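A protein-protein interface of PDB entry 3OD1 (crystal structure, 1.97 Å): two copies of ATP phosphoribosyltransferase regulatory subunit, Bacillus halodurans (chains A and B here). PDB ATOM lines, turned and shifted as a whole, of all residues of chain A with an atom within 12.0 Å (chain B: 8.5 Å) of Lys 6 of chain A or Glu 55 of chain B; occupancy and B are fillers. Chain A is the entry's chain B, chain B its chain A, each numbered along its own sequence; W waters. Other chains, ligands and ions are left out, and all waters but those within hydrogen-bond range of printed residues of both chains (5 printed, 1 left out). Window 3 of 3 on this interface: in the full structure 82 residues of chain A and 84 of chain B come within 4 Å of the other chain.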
ATOM      1  N   MET A   4       2.858   5.426   9.140  1.00  0.00           N
ATOM      2  CA  MET A   4       4.002   4.888   9.871  1.00  0.00           C
ATOM      3  C   MET A   4       5.250   4.798   9.000  1.00  0.00           C
ATOM      4  O   MET A   4       5.173   4.435   7.820  1.00  0.00           O
ATOM      5  CB  MET A   4       3.683   3.507  10.426  1.00  0.00           C
ATOM      6  CG  MET A   4       3.592   2.429   9.373  1.00  0.00           C
ATOM      7  SD  MET A   4       3.042   0.718  10.144  1.00  0.00           S
ATOM      8  CE  MET A   4       1.231   1.205  10.666  1.00  0.00           C
ATOM      9  N   SER A   5       6.398   5.120   9.592  1.00  0.00           N
ATOM     10  CA  SER A   5       7.675   5.077   8.874  1.00  0.00           C
ATOM     11  C   SER A   5       8.156   3.641   8.682  1.00  0.00           C
ATOM     12  O   SER A   5       7.857   2.755   9.486  1.00  0.00           O
ATOM     13  CB  SER A   5       8.754   5.895   9.596  1.00  0.00           C
ATOM     14  OG  SER A   5       8.453   7.279   9.555  1.00  0.00           O
ATOM     15  N   LYS A   6       8.907   3.423   7.610  1.00  0.00           N
ATOM     16  CA  LYS A   6       9.482   2.118   7.361  1.00  0.00           C
ATOM     17  C   LYS A   6      10.465   1.775   8.471  1.00  0.00           C
ATOM     18  O   LYS A   6      11.156   2.652   8.992  1.00  0.00           O
ATOM     19  CB  LYS A   6      10.193   2.117   6.007  1.00  0.00           C
ATOM     20  CG  LYS A   6       9.348   2.681   4.869  1.00  0.00           C
ATOM     21  CD  LYS A   6      10.108   2.638   3.554  1.00  0.00           C
ATOM     22  CE  LYS A   6       9.329   3.305   2.431  1.00  0.00           C
ATOM     23  NZ  LYS A   6       8.058   2.594   2.123  1.00  0.00           N
ATOM     24  N   PRO A   7      10.537   0.492   8.837  1.00  0.00           N
ATOM     25  CA  PRO A   7      11.607   0.033   9.726  1.00  0.00           C
ATOM     26  C   PRO A   7      12.963   0.302   9.078  1.00  0.00           C
ATOM     27  O   PRO A   7      13.033   0.480   7.848  1.00  0.00           O
ATOM     28  CB  PRO A   7      11.371  -1.480   9.800  1.00  0.00           C
ATOM     29  CG  PRO A   7       9.958  -1.682   9.343  1.00  0.00           C
ATOM     30  CD  PRO A   7       9.709  -0.615   8.337  1.00  0.00           C
ATOM     31  N   PHE A   8      14.033   0.344   9.867  1.00  0.00           N
ATOM     32  CA  PHE A   8      15.373   0.458   9.281  1.00  0.00           C
ATOM     33  C   PHE A   8      15.776  -0.917   8.732  1.00  0.00           C
ATOM     34  O   PHE A   8      15.245  -1.952   9.160  1.00  0.00           O
ATOM     35  CB  PHE A   8      16.399   0.955  10.308  1.00  0.00           C
ATOM     36  CG  PHE A   8      16.347   2.442  10.566  1.00  0.00           C
ATOM     37  CD1 PHE A   8      15.220   3.187  10.243  1.00  0.00           C
ATOM     38  CD2 PHE A   8      17.427   3.092  11.154  1.00  0.00           C
ATOM     39  CE1 PHE A   8      15.172   4.559  10.491  1.00  0.00           C
ATOM     40  CE2 PHE A   8      17.382   4.457  11.409  1.00  0.00           C
ATOM     41  CZ  PHE A   8      16.249   5.189  11.075  1.00  0.00           C
ATOM     42  N   MET A   9      16.704  -0.917   7.781  1.00  0.00           N
ATOM     43  CA  MET A   9      17.041  -2.131   7.041  1.00  0.00           C
ATOM     44  C   MET A   9      17.466  -3.296   7.937  1.00  0.00           C
ATOM     45  O   MET A   9      17.206  -4.454   7.618  1.00  0.00           O
ATOM     46  CB  MET A   9      18.105  -1.842   5.972  1.00  0.00           C
ATOM     47  CG  MET A   9      17.622  -0.903   4.851  1.00  0.00           C
ATOM     48  SD  MET A   9      16.025  -1.623   3.918  1.00  0.00           S
ATOM     49  CE  MET A   9      16.817  -3.205   3.059  1.00  0.00           C
ATOM     50  N   PHE A  10      18.098  -2.998   9.068  1.00  0.00           N
ATOM     51  CA  PHE A  10      18.571  -4.059   9.959  1.00  0.00           C
ATOM     52  C   PHE A  10      17.497  -4.599  10.910  1.00  0.00           C
ATOM     53  O   PHE A  10      17.695  -5.636  11.543  1.00  0.00           O
ATOM     54  CB  PHE A  10      19.770  -3.562  10.774  1.00  0.00           C
ATOM     55  CG  PHE A  10      19.421  -2.472  11.745  1.00  0.00           C
ATOM     56  CD1 PHE A  10      19.074  -2.776  13.056  1.00  0.00           C
ATOM     57  CD2 PHE A  10      19.422  -1.140  11.345  1.00  0.00           C
ATOM     58  CE1 PHE A  10      18.744  -1.773  13.956  1.00  0.00           C
ATOM     59  CE2 PHE A  10      19.091  -0.134  12.241  1.00  0.00           C
ATOM     60  CZ  PHE A  10      18.751  -0.454  13.549  1.00  0.00           C
ATOM     61  N   GLU A  11      16.370  -3.898  11.039  1.00  0.00           N
ATOM     62  CA  GLU A  11      15.371  -4.280  12.040  1.00  0.00           C
ATOM     63  C   GLU A  11      14.657  -5.589  11.691  1.00  0.00           C
ATOM     64  O   GLU A  11      14.293  -5.811  10.538  1.00  0.00           O
ATOM     65  CB  GLU A  11      14.368  -3.144  12.259  1.00  0.00           C
ATOM     66  CG  GLU A  11      15.041  -1.822  12.628  1.00  0.00           C
ATOM     67  CD  GLU A  11      14.081  -0.783  13.189  1.00  0.00           C
ATOM     68  OE1 GLU A  11      13.945  -0.718  14.429  1.00  0.00           O
ATOM     69  OE2 GLU A  11      13.477  -0.018  12.399  1.00  0.00           O
ATOM     70  N   LYS A  12      14.498  -6.467  12.687  1.00  0.00           N
ATOM     71  CA  LYS A  12      13.729  -7.706  12.536  1.00  0.00           C
ATOM     72  C   LYS A  12      12.430  -7.527  13.307  1.00  0.00           C
ATOM     73  O   LYS A  12      12.414  -6.853  14.337  1.00  0.00           O
ATOM     74  CB  LYS A  12      14.474  -8.910  13.138  1.00  0.00           C
ATOM     75  CG  LYS A  12      15.747  -9.332  12.391  1.00  0.00           C
ATOM     76  CD  LYS A  12      16.321 -10.654  12.921  1.00  0.00           C
ATOM     77  CE  LYS A  12      16.985 -10.509  14.298  1.00  0.00           C
ATOM     78  NZ  LYS A  12      18.073  -9.485  14.299  1.00  0.00           N
ATOM     79  N   PRO A  13      11.338  -8.146  12.825  1.00  0.00           N
ATOM     80  CA  PRO A  13      10.095  -8.148  13.605  1.00  0.00           C
ATOM     81  C   PRO A  13      10.336  -8.618  15.043  1.00  0.00           C
ATOM     82  O   PRO A  13      11.153  -9.513  15.298  1.00  0.00           O
ATOM     83  CB  PRO A  13       9.216  -9.160  12.865  1.00  0.00           C
ATOM     84  CG  PRO A  13       9.717  -9.146  11.454  1.00  0.00           C
ATOM     85  CD  PRO A  13      11.208  -8.878  11.548  1.00  0.00           C
ATOM     86  N   GLU B  52       9.681 -11.537   8.292  1.00  0.00           N
ATOM     87  CA  GLU B  52      10.505 -10.354   8.030  1.00  0.00           C
ATOM     88  C   GLU B  52       9.556  -9.193   7.759  1.00  0.00           C
ATOM     89  O   GLU B  52       8.389  -9.409   7.426  1.00  0.00           O
ATOM     90  CB  GLU B  52      11.410 -10.556   6.803  1.00  0.00           C
ATOM     91  CG  GLU B  52      12.389 -11.743   6.894  1.00  0.00           C
ATOM     92  CD  GLU B  52      13.722 -11.401   7.574  1.00  0.00           C
ATOM     93  OE1 GLU B  52      13.910 -10.251   8.025  1.00  0.00           O
ATOM     94  OE2 GLU B  52      14.595 -12.295   7.646  1.00  0.00           O
ATOM     95  N   TYR B  53      10.053  -7.967   7.882  1.00  0.00           N
ATOM     96  CA  TYR B  53       9.253  -6.805   7.525  1.00  0.00           C
ATOM     97  C   TYR B  53       9.079  -6.777   6.024  1.00  0.00           C
ATOM     98  O   TYR B  53      10.003  -7.100   5.278  1.00  0.00           O
ATOM     99  CB  TYR B  53       9.930  -5.509   7.977  1.00  0.00           C
ATOM    100  CG  TYR B  53       9.841  -5.262   9.466  1.00  0.00           C
ATOM    101  CD1 TYR B  53       8.616  -4.977  10.067  1.00  0.00           C
ATOM    102  CD2 TYR B  53      10.975  -5.301  10.270  1.00  0.00           C
ATOM    103  CE1 TYR B  53       8.515  -4.752  11.433  1.00  0.00           C
ATOM    104  CE2 TYR B  53      10.885  -5.072  11.653  1.00  0.00           C
ATOM    105  CZ  TYR B  53       9.651  -4.788  12.213  1.00  0.00           C
ATOM    106  OH  TYR B  53       9.556  -4.558  13.556  1.00  0.00           O
ATOM    107  N   TYR B  54       7.886  -6.390   5.592  1.00  0.00           N
ATOM    108  CA  TYR B  54       7.602  -6.176   4.187  1.00  0.00           C
ATOM    109  C   TYR B  54       8.427  -5.014   3.610  1.00  0.00           C
ATOM    110  O   TYR B  54       8.975  -5.125   2.512  1.00  0.00           O
ATOM    111  CB  TYR B  54       6.104  -5.907   3.997  1.00  0.00           C
ATOM    112  CG  TYR B  54       5.775  -5.359   2.632  1.00  0.00           C
ATOM    113  CD1 TYR B  54       5.912  -6.149   1.503  1.00  0.00           C
ATOM    114  CD2 TYR B  54       5.353  -4.042   2.469  1.00  0.00           C
ATOM    115  CE1 TYR B  54       5.632  -5.653   0.239  1.00  0.00           C
ATOM    116  CE2 TYR B  54       5.064  -3.538   1.207  1.00  0.00           C
ATOM    117  CZ  TYR B  54       5.204  -4.350   0.097  1.00  0.00           C
ATOM    118  OH  TYR B  54       4.917  -3.865  -1.161  1.00  0.00           O
ATOM    119  N   GLU B  55       8.510  -3.903   4.343  1.00  0.00           N
ATOM    120  CA  GLU B  55       9.046  -2.653   3.772  1.00  0.00           C
ATOM    121  C   GLU B  55      10.576  -2.645   3.685  1.00  0.00           C
ATOM    122  O   GLU B  55      11.164  -1.754   3.065  1.00  0.00           O
ATOM    123  CB  GLU B  55       8.559  -1.413   4.544  1.00  0.00           C
ATOM    124  CG  GLU B  55       7.063  -1.109   4.434  1.00  0.00           C
ATOM    125  CD  GLU B  55       6.677  -0.649   3.043  1.00  0.00           C
ATOM    126  OE1 GLU B  55       7.581  -0.255   2.278  1.00  0.00           O
ATOM    127  OE2 GLU B  55       5.475  -0.678   2.712  1.00  0.00           O
ATOM    128  N   THR B  56      11.216  -3.623   4.316  1.00  0.00           N
ATOM    129  CA  THR B  56      12.661  -3.781   4.204  1.00  0.00           C
ATOM    130  C   THR B  56      12.981  -4.989   3.334  1.00  0.00           C
ATOM    131  O   THR B  56      13.203  -4.865   2.128  1.00  0.00           O
ATOM    132  CB  THR B  56      13.331  -3.904   5.581  1.00  0.00           C
ATOM    133  OG1 THR B  56      12.754  -4.992   6.314  1.00  0.00           O
ATOM    134  CG2 THR B  56      13.125  -2.631   6.372  1.00  0.00           C
ATOM    135  N   VAL B  57      12.939  -6.162   3.947  1.00  0.00           N
ATOM    136  CA  VAL B  57      13.274  -7.416   3.291  1.00  0.00           C
ATOM    137  C   VAL B  57      12.329  -7.834   2.172  1.00  0.00           C
ATOM    138  O   VAL B  57      12.771  -8.285   1.110  1.00  0.00           O
ATOM    139  CB  VAL B  57      13.387  -8.524   4.359  1.00  0.00           C
ATOM    140  CG1 VAL B  57      13.435  -9.887   3.721  1.00  0.00           C
ATOM    141  CG2 VAL B  57      14.626  -8.256   5.211  1.00  0.00           C
ATOM    142  N   GLY B  58      11.028  -7.674   2.393  1.00  0.00           N
ATOM    143  CA  GLY B  58      10.064  -8.104   1.404  1.00  0.00           C
ATOM    144  C   GLY B  58      10.215  -7.392   0.066  1.00  0.00           C
ATOM    145  O   GLY B  58      10.178  -8.017  -0.993  1.00  0.00           O
ATOM    146  N   VAL B  59      10.387  -6.081   0.110  1.00  0.00           N
ATOM    147  CA  VAL B  59      10.456  -5.311  -1.118  1.00  0.00           C
ATOM    148  C   VAL B  59      11.758  -5.511  -1.903  1.00  0.00           C
ATOM    149  O   VAL B  59      11.787  -5.280  -3.102  1.00  0.00           O
ATOM    150  CB  VAL B  59      10.177  -3.801  -0.881  1.00  0.00           C
ATOM    151  CG1 VAL B  59       8.759  -3.598  -0.390  1.00  0.00           C
ATOM    152  CG2 VAL B  59      11.158  -3.216   0.112  1.00  0.00           C
ATOM    153  N   VAL B  60      12.833  -5.948  -1.252  1.00  0.00           N
ATOM    154  CA  VAL B  60      14.093  -6.097  -1.978  1.00  0.00           C
ATOM    155  C   VAL B  60      14.318  -7.527  -2.438  1.00  0.00           C
ATOM    156  O   VAL B  60      15.286  -7.810  -3.115  1.00  0.00           O
ATOM    157  CB  VAL B  60      15.319  -5.590  -1.181  1.00  0.00           C
ATOM    158  CG1 VAL B  60      15.169  -4.093  -0.861  1.00  0.00           C
ATOM    159  CG2 VAL B  60      15.521  -6.424   0.079  1.00  0.00           C
ATOM    160  N   ASP B  65       5.990  -8.413  -6.040  1.00  0.00           N
ATOM    161  CA  ASP B  65       5.152  -7.955  -4.947  1.00  0.00           C
ATOM    162  C   ASP B  65       3.871  -8.767  -4.790  1.00  0.00           C
ATOM    163  O   ASP B  65       3.467  -9.098  -3.679  1.00  0.00           O
ATOM    164  CB  ASP B  65       4.798  -6.481  -5.120  1.00  0.00           C
ATOM    165  CG  ASP B  65       4.240  -5.884  -3.850  1.00  0.00           C
ATOM    166  OD1 ASP B  65       5.045  -5.565  -2.952  1.00  0.00           O
ATOM    167  OD2 ASP B  65       3.003  -5.746  -3.746  1.00  0.00           O
ATOM    168  N   LEU B  68       4.171 -12.118  -2.895  1.00  0.00           N
ATOM    169  CA  LEU B  68       4.557 -12.139  -1.484  1.00  0.00           C
ATOM    170  C   LEU B  68       3.413 -12.549  -0.567  1.00  0.00           C
ATOM    171  O   LEU B  68       2.264 -12.143  -0.762  1.00  0.00           O
ATOM    172  CB  LEU B  68       5.092 -10.774  -1.025  1.00  0.00           C
ATOM    173  CG  LEU B  68       6.317 -10.236  -1.759  1.00  0.00           C
ATOM    174  CD1 LEU B  68       6.565  -8.756  -1.406  1.00  0.00           C
ATOM    175  CD2 LEU B  68       7.539 -11.093  -1.469  1.00  0.00           C
ATOM    176  N   LYS B  70       1.945 -11.571   2.458  1.00  0.00           N
ATOM    177  CA  LYS B  70       1.861 -10.433   3.362  1.00  0.00           C
ATOM    178  C   LYS B  70       0.869 -10.685   4.502  1.00  0.00           C
ATOM    179  O   LYS B  70      -0.154 -11.352   4.315  1.00  0.00           O
ATOM    180  CB  LYS B  70       1.403  -9.196   2.586  1.00  0.00           C
ATOM    181  CG  LYS B  70       2.325  -8.780   1.435  1.00  0.00           C
ATOM    182  CD  LYS B  70       1.690  -7.581   0.708  1.00  0.00           C
ATOM    183  CE  LYS B  70       2.435  -7.190  -0.552  1.00  0.00           C
ATOM    184  NZ  LYS B  70       1.796  -5.974  -1.168  1.00  0.00           N
ATOM    185  N   ASN B  77       2.037  -3.336  11.527  1.00  0.00           N
ATOM    186  CA  ASN B  77       3.136  -3.434  10.567  1.00  0.00           C
ATOM    187  C   ASN B  77       2.812  -4.505   9.547  1.00  0.00           C
ATOM    188  O   ASN B  77       2.254  -5.529   9.897  1.00  0.00           O
ATOM    189  CB  ASN B  77       4.452  -3.823  11.240  1.00  0.00           C
ATOM    190  CG  ASN B  77       4.873  -2.861  12.328  1.00  0.00           C
ATOM    191  OD1 ASN B  77       5.028  -1.663  12.089  1.00  0.00           O
ATOM    192  ND2 ASN B  77       5.095  -3.390  13.532  1.00  0.00           N
ATOM    193  N   THR B  78       3.203  -4.298   8.311  1.00  0.00           N
ATOM    194  CA  THR B  78       3.090  -5.329   7.316  1.00  0.00           C
ATOM    195  C   THR B  78       4.332  -6.219   7.333  1.00  0.00           C
ATOM    196  O   THR B  78       5.429  -5.761   7.180  1.00  0.00           O
ATOM    197  CB  THR B  78       2.791  -4.775   5.892  1.00  0.00           C
ATOM    198  OG1 THR B  78       1.641  -3.945   5.929  1.00  0.00           O
ATOM    199  CG2 THR B  78       2.509  -5.887   4.951  1.00  0.00           C
ATOM    200  N   LEU B  79       4.116  -7.502   7.555  1.00  0.00           N
ATOM    201  CA  LEU B  79       5.180  -8.464   7.513  1.00  0.00           C
ATOM    202  C   LEU B  79       5.029  -9.368   6.331  1.00  0.00           C
ATOM    203  O   LEU B  79       3.999  -9.449   5.763  1.00  0.00           O
ATOM    204  CB  LEU B  79       5.198  -9.320   8.760  1.00  0.00           C
ATOM    205  CG  LEU B  79       5.115  -8.660  10.113  1.00  0.00           C
ATOM    206  CD1 LEU B  79       5.124  -9.694  11.126  1.00  0.00           C
ATOM    207  CD2 LEU B  79       6.222  -7.725  10.337  1.00  0.00           C
ATOM    208  N   VAL B  80       6.083 -10.083   6.004  1.00  0.00           N
ATOM    209  CA  VAL B  80       6.003 -11.170   5.064  1.00  0.00           C
ATOM    210  C   VAL B  80       6.506 -12.443   5.697  1.00  0.00           C
ATOM    211  O   VAL B  80       7.388 -12.411   6.485  1.00  0.00           O
ATOM    212  CB  VAL B  80       6.737 -10.899   3.735  1.00  0.00           C
ATOM    213  CG1 VAL B  80       6.108  -9.801   2.995  1.00  0.00           C
ATOM    214  CG2 VAL B  80       8.161 -10.663   3.924  1.00  0.00           C
ATOM    215  N   PHE B 307      21.376  -2.833   2.313  1.00  0.00           N
ATOM    216  CA  PHE B 307      21.528  -3.024   3.739  1.00  0.00           C
ATOM    217  C   PHE B 307      22.759  -2.287   4.295  1.00  0.00           C
ATOM    218  O   PHE B 307      23.250  -2.618   5.375  1.00  0.00           O
ATOM    219  CB  PHE B 307      21.613  -4.521   4.056  1.00  0.00           C
ATOM    220  CG  PHE B 307      20.341  -5.257   3.779  1.00  0.00           C
ATOM    221  CD1 PHE B 307      19.397  -5.446   4.793  1.00  0.00           C
ATOM    222  CD2 PHE B 307      20.065  -5.731   2.500  1.00  0.00           C
ATOM    223  CE1 PHE B 307      18.197  -6.101   4.540  1.00  0.00           C
ATOM    224  CE2 PHE B 307      18.870  -6.407   2.245  1.00  0.00           C
ATOM    225  CZ  PHE B 307      17.932  -6.582   3.271  1.00  0.00           C
HETATM  226  O   HOH W   1       7.468   0.206  -0.173  1.00  0.00           O
HETATM  227  O   HOH W   2      12.831  -7.835   8.556  1.00  0.00           O
HETATM  228  O   HOH W   3      14.858  -5.540   7.959  1.00  0.00           O
HETATM  229  O   HOH W   4      11.716  -4.023  15.015  1.00  0.00           O
HETATM  230  O   HOH W   5       6.594  -0.481  10.331  1.00  0.00           O
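The side-chain amino group (NZ) of Lys 6 of chain A is in salt-bridge range of the side-chain carboxylate (OE1) of Glu 55 of chain B, at 2.9 Å. The side-chain amide oxygen of Asn 77 of chain B sits close to the side-chain sulfur of Met 4 of chain A, at 3.7 Å.
O of Glu 52 of chain B is in hydrogen-bond range of N of Val 80 of chain B, at 2.8 Å. The backbone carbonyl oxygen of Tyr 53 of chain B is in hydrogen-bond range of the backbone NH of Gly 58 of chain B, 3.1 Å away. The side-chain carboxylate (OE2) of Glu 11 of chain A lies within hydrogen-bond range of the backbone NH (N) of Phe 8 of chain A (2.6 Å).
CG of Pro 7 of chain A touches CG of Tyr 53 of chain B (3.6 Å). CG2 of Thr 56 of chain B touches O of Pro 7 of chain A (3.4 Å). CG2 of Thr 56 of chain B touches O of Phe 8 of chain A (3.6 Å). CB of Thr 56 of chain B touches SD of Met 9 of chain A (3.9 Å). CE of Met 9 of chain A touches CE1 of Phe 307 of chain B (3.5 Å). Glu 11 of chain A touches Tyr 53 of chain B (O to CD2, 3.4 Å). Lys 12 of chain A touches Tyr 53 of chain B (C to CE2, 3.3 Å). Pro 13 of chain A touches Glu 52 of chain B. Pro 13 of chain A touches Tyr 53 of chain B (N to CE2, 3.3 Å). Pro 13 of chain A touches Leu 79 of chain B.
No residue of chain B comes within 4 Å of Ser 5 of chain A. Lys 6 of chain A touches one residue of chain B. Pro 7 of chain A touches just these residues of chain B: Tyr 53 and Thr 56. Of the printed residues of chain B, Phe 8 of chain A touches Thr 56 (3.6 Å). Phe 10 of chain A touches none of the printed residues of chain B. Printed residues of chain B within 4 Å of Glu 11 of chain A: Tyr 53. Printed residues of chain B within 4 Å of Pro 13 of chain A: Glu 52, Tyr 53 and Leu 79. Of the printed residues of chain A, Tyr 53 of chain B touches Pro 7 (3.6 Å), Glu 11 (3.4 Å), Lys 12 (3.3 Å) and Pro 13 (3.3 Å). No residue of chain A comes within 4 Å of Tyr 54 of chain B. Glu 55 of chain B touches just one residue of chain A: Lys 6 (2.9 Å). Thr 56 of chain B touches just these residues of chain A: Pro 7 (3.4 Å), Phe 8 (3.6 Å) and Met 9 (3.9 Å). No residue of chain A comes within 4 Å of Gly 58 of chain B. No residue of chain A comes within 4 Å of Val 59 of chain B. Lys 70 of chain B touches none of the printed residues of chain A. No residue of chain A comes within 4 Å of Thr 78 of chain B. Of the printed residues of chain A, Leu 79 of chain B touches Pro 13. The nearest residue of chain B that does not touch Lys 6 of chain A is Thr 56 of chain B (5.6 Å). The nearest residue of chain A that does not touch Glu 55 of chain B is Pro 7 of chain A (4.04 Å). The nearest printed residue of chain A that does not touch Tyr 53 of chain B is Phe 8 of chain A (5.5 Å).
Printed residues of chain A that touch a printed residue of chain B: Met 4, Lys 6, Pro 7, Phe 8, Met 9, Glu 11, Lys 12 and Pro 13. Hydrophobic or aromatic side chains of chain A that line the printed part of chain B: Met 4, Pro 7, Met 9 and Pro 13. Hydrophobic or aromatic side chains of chain B within 4 Å of the printed part of chain A: Tyr 53, Leu 79 and Phe 307.
No position is printed for both chains. Of the 12 pairs that touch across the chains among the printed residues, none has its exchanged pair printed and touching as well.
Water W1 bridges the side-chain carboxylate (OE1) of Glu 55 of chain B and the side-chain amino group (NZ) of Lys 6 of chain A. Water W3 lies within hydrogen-bond range of the backbone carbonyl oxygen of Met 9 of chain A (2.6 Å), the backbone carbonyl oxygen of Glu 11 of chain A (2.7 Å) and the side-chain hydroxyl of Thr 56 of chain B (2.7 Å). Water W5 lies within hydrogen-bond range of OD1 of Asn 77 of chain B and SD of Met 4 of chain A. Water W4 lies within hydrogen-bond range of OH of Tyr 53 of chain B (2.7 Å) and O of Lys 12 of chain A (3.0 Å). Water W2 lies within hydrogen-bond range of the side-chain carboxylate of Glu 52 of chain B (2.7 Å), the backbone NH of Tyr 53 of chain B (2.9 Å) and the backbone carbonyl oxygen of Glu 11 of chain A (3.2 Å).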
